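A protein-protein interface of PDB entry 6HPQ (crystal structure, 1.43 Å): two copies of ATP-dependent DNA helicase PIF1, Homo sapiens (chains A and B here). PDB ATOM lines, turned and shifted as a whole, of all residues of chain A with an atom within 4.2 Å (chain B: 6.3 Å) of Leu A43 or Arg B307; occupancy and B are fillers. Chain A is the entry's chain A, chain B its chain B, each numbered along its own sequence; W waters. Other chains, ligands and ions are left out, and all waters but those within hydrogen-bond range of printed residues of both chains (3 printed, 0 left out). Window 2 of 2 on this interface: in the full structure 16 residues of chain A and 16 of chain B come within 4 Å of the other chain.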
ATOM      1  N   LEU A  17       0.593   3.045  32.672  1.00  0.00           N
ATOM      2  CA  LEU A  17       1.618   3.956  32.104  1.00  0.00           C
ATOM      3  C   LEU A  17       2.909   4.004  32.921  1.00  0.00           C
ATOM      4  O   LEU A  17       3.949   4.386  32.380  1.00  0.00           O
ATOM      5  CB  LEU A  17       1.026   5.339  31.871  1.00  0.00           C
ATOM      6  CG  LEU A  17      -0.093   5.421  30.843  1.00  0.00           C
ATOM      7  CD1 LEU A  17      -0.671   6.835  30.790  1.00  0.00           C
ATOM      8  CD2 LEU A  17       0.338   4.970  29.491  1.00  0.00           C
ATOM      9  N   ILE A  39      -6.720   2.637  27.363  1.00  0.00           N
ATOM     10  CA  ILE A  39      -5.318   2.231  27.621  1.00  0.00           C
ATOM     11  C   ILE A  39      -4.611   2.078  26.282  1.00  0.00           C
ATOM     12  O   ILE A  39      -3.495   2.571  26.131  1.00  0.00           O
ATOM     13  CB  ILE A  39      -5.314   0.954  28.473  1.00  0.00           C
ATOM     14  CG1 ILE A  39      -5.642   1.242  29.929  1.00  0.00           C
ATOM     15  CG2 ILE A  39      -3.988   0.227  28.335  1.00  0.00           C
ATOM     16  CD1 ILE A  39      -6.098  -0.009  30.661  1.00  0.00           C
ATOM     17  N   LEU A  40      -5.216   1.349  25.366  1.00  0.00           N
ATOM     18  CA  LEU A  40      -4.616   1.138  24.040  1.00  0.00           C
ATOM     19  C   LEU A  40      -4.353   2.483  23.353  1.00  0.00           C
ATOM     20  O   LEU A  40      -3.294   2.643  22.707  1.00  0.00           O
ATOM     21  CB  LEU A  40      -5.525   0.209  23.238  1.00  0.00           C
ATOM     22  CG  LEU A  40      -5.564  -1.241  23.700  1.00  0.00           C
ATOM     23  CD1 LEU A  40      -6.687  -2.027  23.015  1.00  0.00           C
ATOM     24  CD2 LEU A  40      -4.208  -1.904  23.493  1.00  0.00           C
ATOM     25  N   GLY A  41      -5.269   3.425  23.467  1.00  0.00           N
ATOM     26  CA  GLY A  41      -5.125   4.772  22.906  1.00  0.00           C
ATOM     27  C   GLY A  41      -3.968   5.516  23.514  1.00  0.00           C
ATOM     28  O   GLY A  41      -3.406   6.404  22.858  1.00  0.00           O
ATOM     29  N   SER A  42      -3.625   5.194  24.743  1.00  0.00           N
ATOM     30  CA  SER A  42      -2.620   5.939  25.532  1.00  0.00           C
ATOM     31  C   SER A  42      -1.224   5.343  25.366  1.00  0.00           C
ATOM     32  O   SER A  42      -0.267   5.940  25.905  1.00  0.00           O
ATOM     33  CB  SER A  42      -3.005   5.878  26.991  1.00  0.00           C
ATOM     34  OG  SER A  42      -4.187   6.613  27.271  1.00  0.00           O
ATOM     35  N   LEU A  43      -1.103   4.224  24.656  1.00  0.00           N
ATOM     36  CA  LEU A  43       0.193   3.511  24.489  1.00  0.00           C
ATOM     37  C   LEU A  43       0.626   3.590  23.034  1.00  0.00           C
ATOM     38  O   LEU A  43      -0.219   3.566  22.155  1.00  0.00           O
ATOM     39  CB  LEU A  43       0.001   2.026  24.886  1.00  0.00           C
ATOM     40  CG  LEU A  43      -0.215   1.745  26.363  1.00  0.00           C
ATOM     41  CD1 LEU A  43      -0.667   0.302  26.519  1.00  0.00           C
ATOM     42  CD2 LEU A  43       1.054   2.014  27.168  1.00  0.00           C
ATOM     43  N   PRO A  44       1.937   3.499  22.741  1.00  0.00           N
ATOM     44  CA  PRO A  44       2.404   3.281  21.365  1.00  0.00           C
ATOM     45  C   PRO A  44       1.803   1.996  20.844  1.00  0.00           C
ATOM     46  O   PRO A  44       1.683   1.014  21.606  1.00  0.00           O
ATOM     47  CB  PRO A  44       3.924   3.077  21.485  1.00  0.00           C
ATOM     48  CG  PRO A  44       4.288   3.381  22.927  1.00  0.00           C
ATOM     49  CD  PRO A  44       3.012   3.429  23.739  1.00  0.00           C
ATOM     50  N   PRO A  45       1.443   1.902  19.552  1.00  0.00           N
ATOM     51  CA  PRO A  45       0.960   0.633  19.052  1.00  0.00           C
ATOM     52  C   PRO A  45       2.098  -0.386  18.923  1.00  0.00           C
ATOM     53  O   PRO A  45       1.799  -1.593  19.052  1.00  0.00           O
ATOM     54  CB  PRO A  45       0.275   1.015  17.739  1.00  0.00           C
ATOM     55  CG  PRO A  45       1.039   2.238  17.276  1.00  0.00           C
ATOM     56  CD  PRO A  45       1.328   2.983  18.551  1.00  0.00           C
ATOM     57  N   THR A  48       2.650  -3.327  21.575  1.00  0.00           N
ATOM     58  CA  THR A  48       1.391  -3.431  22.351  1.00  0.00           C
ATOM     59  C   THR A  48       0.499  -4.408  21.619  1.00  0.00           C
ATOM     60  O   THR A  48       0.175  -4.129  20.457  1.00  0.00           O
ATOM     61  CB  THR A  48       0.697  -2.073  22.564  1.00  0.00           C
ATOM     62  OG1 THR A  48       1.644  -1.173  23.170  1.00  0.00           O
ATOM     63  CG2 THR A  48      -0.541  -2.189  23.413  1.00  0.00           C
ATOM     64  N   ARG A 100       3.931  -5.307  25.845  1.00  0.00           N
ATOM     65  CA  ARG A 100       2.716  -5.167  26.651  1.00  0.00           C
ATOM     66  C   ARG A 100       1.633  -6.050  26.048  1.00  0.00           C
ATOM     67  O   ARG A 100       1.350  -5.949  24.831  1.00  0.00           O
ATOM     68  CB  ARG A 100       2.234  -3.724  26.634  1.00  0.00           C
ATOM     69  CG  ARG A 100       3.223  -2.737  27.256  1.00  0.00           C
ATOM     70  CD  ARG A 100       2.973  -1.262  26.943  1.00  0.00           C
ATOM     71  NE  ARG A 100       3.301  -1.062  25.554  1.00  0.00           N
ATOM     72  CZ  ARG A 100       4.499  -0.809  25.088  1.00  0.00           C
ATOM     73  NH1 ARG A 100       5.520  -0.692  25.916  1.00  0.00           N
ATOM     74  NH2 ARG A 100       4.706  -0.749  23.786  1.00  0.00           N
ATOM     75  N   HIS B 246       8.077  15.638  18.325  1.00  0.00           N
ATOM     76  CA  HIS B 246       7.215  14.564  18.869  1.00  0.00           C
ATOM     77  C   HIS B 246       7.169  13.443  17.828  1.00  0.00           C
ATOM     78  O   HIS B 246       6.819  13.730  16.689  1.00  0.00           O
ATOM     79  CB  HIS B 246       5.843  15.157  19.134  1.00  0.00           C
ATOM     80  CG  HIS B 246       5.818  16.127  20.261  1.00  0.00           C
ATOM     81  ND1 HIS B 246       6.298  17.414  20.183  1.00  0.00           N
ATOM     82  CD2 HIS B 246       5.363  15.956  21.522  1.00  0.00           C
ATOM     83  CE1 HIS B 246       6.140  18.002  21.364  1.00  0.00           C
ATOM     84  NE2 HIS B 246       5.557  17.127  22.189  1.00  0.00           N
ATOM     85  N   ARG B 247       7.325  12.204  18.248  1.00  0.00           N
ATOM     86  CA  ARG B 247       7.482  11.040  17.352  1.00  0.00           C
ATOM     87  C   ARG B 247       6.259  10.132  17.514  1.00  0.00           C
ATOM     88  O   ARG B 247       5.864   9.883  18.680  1.00  0.00           O
ATOM     89  CB  ARG B 247       8.797  10.357  17.740  1.00  0.00           C
ATOM     90  CG  ARG B 247       8.962   8.935  17.252  1.00  0.00           C
ATOM     91  CD  ARG B 247      10.264   8.356  17.768  1.00  0.00           C
ATOM     92  NE  ARG B 247      11.348   8.990  17.045  1.00  0.00           N
ATOM     93  CZ  ARG B 247      12.181   8.359  16.234  1.00  0.00           C
ATOM     94  NH1 ARG B 247      12.084   7.054  16.070  1.00  0.00           N
ATOM     95  NH2 ARG B 247      13.113   9.042  15.597  1.00  0.00           N
ATOM     96  N   PHE B 248       5.751   9.598  16.426  1.00  0.00           N
ATOM     97  CA  PHE B 248       4.642   8.624  16.408  1.00  0.00           C
ATOM     98  C   PHE B 248       5.058   7.520  15.446  1.00  0.00           C
ATOM     99  O   PHE B 248       5.120   7.767  14.246  1.00  0.00           O
ATOM    100  CB  PHE B 248       3.311   9.282  16.020  1.00  0.00           C
ATOM    101  CG  PHE B 248       2.951  10.444  16.904  1.00  0.00           C
ATOM    102  CD1 PHE B 248       3.432  11.701  16.595  1.00  0.00           C
ATOM    103  CD2 PHE B 248       2.288  10.276  18.099  1.00  0.00           C
ATOM    104  CE1 PHE B 248       3.192  12.776  17.419  1.00  0.00           C
ATOM    105  CE2 PHE B 248       2.044  11.363  18.916  1.00  0.00           C
ATOM    106  CZ  PHE B 248       2.494  12.610  18.573  1.00  0.00           C
ATOM    107  N   GLU B 249       5.356   6.353  15.964  1.00  0.00           N
ATOM    108  CA  GLU B 249       5.878   5.222  15.171  1.00  0.00           C
ATOM    109  C   GLU B 249       4.686   4.365  14.762  1.00  0.00           C
ATOM    110  O   GLU B 249       3.854   4.003  15.609  1.00  0.00           O
ATOM    111  CB  GLU B 249       6.946   4.438  15.959  1.00  0.00           C
ATOM    112  CG  GLU B 249       8.206   5.270  16.288  1.00  0.00           C
ATOM    113  CD  GLU B 249       9.253   4.625  17.191  1.00  0.00           C
ATOM    114  OE1 GLU B 249       9.104   3.421  17.478  1.00  0.00           O
ATOM    115  OE2 GLU B 249      10.224   5.336  17.589  1.00  0.00           O
ATOM    116  N   ALA B 250       4.592   4.000  13.498  1.00  0.00           N
ATOM    117  CA  ALA B 250       3.509   3.115  13.029  1.00  0.00           C
ATOM    118  C   ALA B 250       3.746   1.672  13.496  1.00  0.00           C
ATOM    119  O   ALA B 250       4.921   1.269  13.741  1.00  0.00           O
ATOM    120  CB  ALA B 250       3.464   3.177  11.519  1.00  0.00           C
ATOM    121  N   GLU B 303      -1.442  16.960  23.518  1.00  0.00           N
ATOM    122  CA  GLU B 303      -2.029  16.591  24.815  1.00  0.00           C
ATOM    123  C   GLU B 303      -0.890  16.322  25.810  1.00  0.00           C
ATOM    124  O   GLU B 303       0.153  15.825  25.425  1.00  0.00           O
ATOM    125  CB  GLU B 303      -2.921  15.371  24.634  1.00  0.00           C
ATOM    126  CG  GLU B 303      -4.148  15.624  23.803  1.00  0.00           C
ATOM    127  CD  GLU B 303      -5.250  14.612  24.056  1.00  0.00           C
ATOM    128  OE1 GLU B 303      -6.368  15.047  24.344  1.00  0.00           O
ATOM    129  OE2 GLU B 303      -4.986  13.390  23.927  1.00  0.00           O
ATOM    130  N   GLU B 305      -1.156  14.143  28.325  1.00  0.00           N
ATOM    131  CA  GLU B 305      -1.373  12.776  28.856  1.00  0.00           C
ATOM    132  C   GLU B 305      -1.053  11.732  27.782  1.00  0.00           C
ATOM    133  O   GLU B 305      -1.133  12.044  26.540  1.00  0.00           O
ATOM    134  CB  GLU B 305      -2.831  12.599  29.315  1.00  0.00           C
ATOM    135  CG  GLU B 305      -3.610  13.895  29.574  1.00  0.00           C
ATOM    136  CD  GLU B 305      -4.086  14.711  28.361  1.00  0.00           C
ATOM    137  OE1 GLU B 305      -5.080  14.310  27.712  1.00  0.00           O
ATOM    138  OE2 GLU B 305      -3.538  15.766  28.151  1.00  0.00           O
ATOM    139  N   GLY B 306      -0.774  10.503  28.188  1.00  0.00           N
ATOM    140  CA  GLY B 306      -0.690   9.365  27.258  1.00  0.00           C
ATOM    141  C   GLY B 306       0.400   9.572  26.241  1.00  0.00           C
ATOM    142  O   GLY B 306       1.544   9.949  26.605  1.00  0.00           O
ATOM    143  N   ARG B 307       0.071   9.364  24.976  1.00  0.00           N
ATOM    144  CA  ARG B 307       1.050   9.459  23.869  1.00  0.00           C
ATOM    145  C   ARG B 307       1.350  10.912  23.523  1.00  0.00           C
ATOM    146  O   ARG B 307       2.232  11.137  22.666  1.00  0.00           O
ATOM    147  CB  ARG B 307       0.449   8.850  22.595  1.00  0.00           C
ATOM    148  CG  ARG B 307       0.160   7.362  22.696  1.00  0.00           C
ATOM    149  CD  ARG B 307      -0.358   6.834  21.376  1.00  0.00           C
ATOM    150  NE  ARG B 307       0.695   6.830  20.352  1.00  0.00           N
ATOM    151  CZ  ARG B 307       0.485   6.610  19.063  1.00  0.00           C
ATOM    152  NH1 ARG B 307      -0.748   6.364  18.627  1.00  0.00           N
ATOM    153  NH2 ARG B 307       1.527   6.613  18.242  1.00  0.00           N
ATOM    154  N   GLY B 308       0.613  11.863  24.083  1.00  0.00           N
ATOM    155  CA  GLY B 308       0.787  13.269  23.695  1.00  0.00           C
ATOM    156  C   GLY B 308       0.325  13.502  22.279  1.00  0.00           C
ATOM    157  O   GLY B 308       1.078  14.048  21.462  1.00  0.00           O
ATOM    158  N   LEU B 309      -0.896  13.094  21.990  1.00  0.00           N
ATOM    159  CA  LEU B 309      -1.469  13.232  20.631  1.00  0.00           C
ATOM    160  C   LEU B 309      -1.531  14.695  20.214  1.00  0.00           C
ATOM    161  O   LEU B 309      -1.828  15.570  21.012  1.00  0.00           O
ATOM    162  CB  LEU B 309      -2.869  12.626  20.596  1.00  0.00           C
ATOM    163  CG  LEU B 309      -2.907  11.115  20.778  1.00  0.00           C
ATOM    164  CD1 LEU B 309      -4.327  10.629  20.981  1.00  0.00           C
ATOM    165  CD2 LEU B 309      -2.248  10.426  19.585  1.00  0.00           C
ATOM    166  N   HIS B 323      -6.488  11.216  16.674  1.00  0.00           N
ATOM    167  CA  HIS B 323      -6.305   9.879  17.297  1.00  0.00           C
ATOM    168  C   HIS B 323      -5.801   8.896  16.233  1.00  0.00           C
ATOM    169  O   HIS B 323      -5.868   9.221  14.999  1.00  0.00           O
ATOM    170  CB  HIS B 323      -7.604   9.408  17.973  1.00  0.00           C
ATOM    171  CG  HIS B 323      -8.040  10.256  19.116  1.00  0.00           C
ATOM    172  ND1 HIS B 323      -8.881  11.360  18.971  1.00  0.00           N
ATOM    173  CD2 HIS B 323      -7.773  10.166  20.433  1.00  0.00           C
ATOM    174  CE1 HIS B 323      -9.132  11.881  20.154  1.00  0.00           C
ATOM    175  NE2 HIS B 323      -8.449  11.185  21.064  1.00  0.00           N
ATOM    176  N   ALA B 324      -5.291   7.740  16.655  1.00  0.00           N
ATOM    177  CA  ALA B 324      -4.819   6.661  15.763  1.00  0.00           C
ATOM    178  C   ALA B 324      -5.918   6.232  14.795  1.00  0.00           C
ATOM    179  O   ALA B 324      -7.112   6.193  15.138  1.00  0.00           O
ATOM    180  CB  ALA B 324      -4.436   5.466  16.600  1.00  0.00           C
ATOM    181  N   GLN B 341      -1.403   4.071  12.548  1.00  0.00           N
ATOM    182  CA  GLN B 341      -0.651   5.348  12.601  1.00  0.00           C
ATOM    183  C   GLN B 341      -1.672   6.470  12.731  1.00  0.00           C
ATOM    184  O   GLN B 341      -2.867   6.219  12.417  1.00  0.00           O
ATOM    185  CB  GLN B 341       0.161   5.489  11.307  1.00  0.00           C
ATOM    186  CG  GLN B 341       1.013   6.734  11.115  1.00  0.00           C
ATOM    187  CD  GLN B 341       2.072   6.959  12.167  1.00  0.00           C
ATOM    188  OE1 GLN B 341       3.312   6.795  11.935  1.00  0.00           O
ATOM    189  NE2 GLN B 341       1.597   7.306  13.338  1.00  0.00           N
ATOM    190  N   LEU B 342      -1.234   7.671  13.119  1.00  0.00           N
ATOM    191  CA  LEU B 342      -2.133   8.847  13.052  1.00  0.00           C
ATOM    192  C   LEU B 342      -2.368   9.151  11.590  1.00  0.00           C
ATOM    193  O   LEU B 342      -1.442   9.085  10.792  1.00  0.00           O
ATOM    194  CB  LEU B 342      -1.482  10.053  13.725  1.00  0.00           C
ATOM    195  CG  LEU B 342      -0.978   9.865  15.153  1.00  0.00           C
ATOM    196  CD1 LEU B 342      -0.607  11.215  15.754  1.00  0.00           C
ATOM    197  CD2 LEU B 342      -2.007   9.176  15.996  1.00  0.00           C
HETATM  198  O   HOH W   1      -3.193   6.048  20.137  1.00  0.00           O
HETATM  199  O   HOH W   2      -2.682   9.218  24.161  1.00  0.00           O
HETATM  200  O   HOH W   3      -3.848   9.001  28.641  1.00  0.00           O
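No position is printed for both chains.
Water W1 bridges the backbone carbonyl oxygen (O) of Gly A41 and the guanidinium group (NH1) of Arg B307.
Water W3 bridges OG of Ser A42 (2.8 Å) and N of Gly B306 (3.5 Å).
Water W2 bridges the backbone NH of Arg B307 and the backbone carbonyl oxygen of Gly A41.
Of the printed residues of chain B, Gly A41 touches Arg B307 (3.4 Å).
Of the printed residues of chain B, Ser A42 touches Gly B306 (3.7 Å) and Arg B307 (3.5 Å).
Printed residues of chain B within 4 Å of Leu A43: Arg B307.
Of the printed residues of chain B, Pro A45 touches Glu B249 and Arg B307.
Printed residues of chain A within 4 Å of Glu B249: Pro A45 (3.7 Å).
Printed residues of chain A within 4 Å of Gly B306: Ser A42 (3.7 Å).
Of chain A, only Gly A41 (3.4 Å), Ser A42 (3.5 Å), Leu A43 (3.4 Å) and Pro A45 (3.6 Å) come within 4 Å of Arg B307.
Ala B324 touches none of the printed residues of chain A.
Of the 10 printed residues of chain A, 4 touch a printed residue of chain B.
Hydrophobic or aromatic side chains of chain A within 4 Å of the printed part of chain B: Pro A45.
Among the printed residues, 6 pairs touch across the chains.
Among the printed residues, no Asp or Glu carboxylate lies within 4 Å of a Lys or Arg side-chain nitrogen of the other chain.
Among the printed residues, merely in contact across the chains: Gly A41 with Arg B307, Ser A42 with Gly B306, Ser A42 with Arg B307, Leu A43 with Arg B307, Pro A45 with Glu B249 and Pro A45 with Arg B307.
The guanidinium group (NH1) of Arg B247 is in salt-bridge range of the side-chain carboxylate (OE2) of Glu B249.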
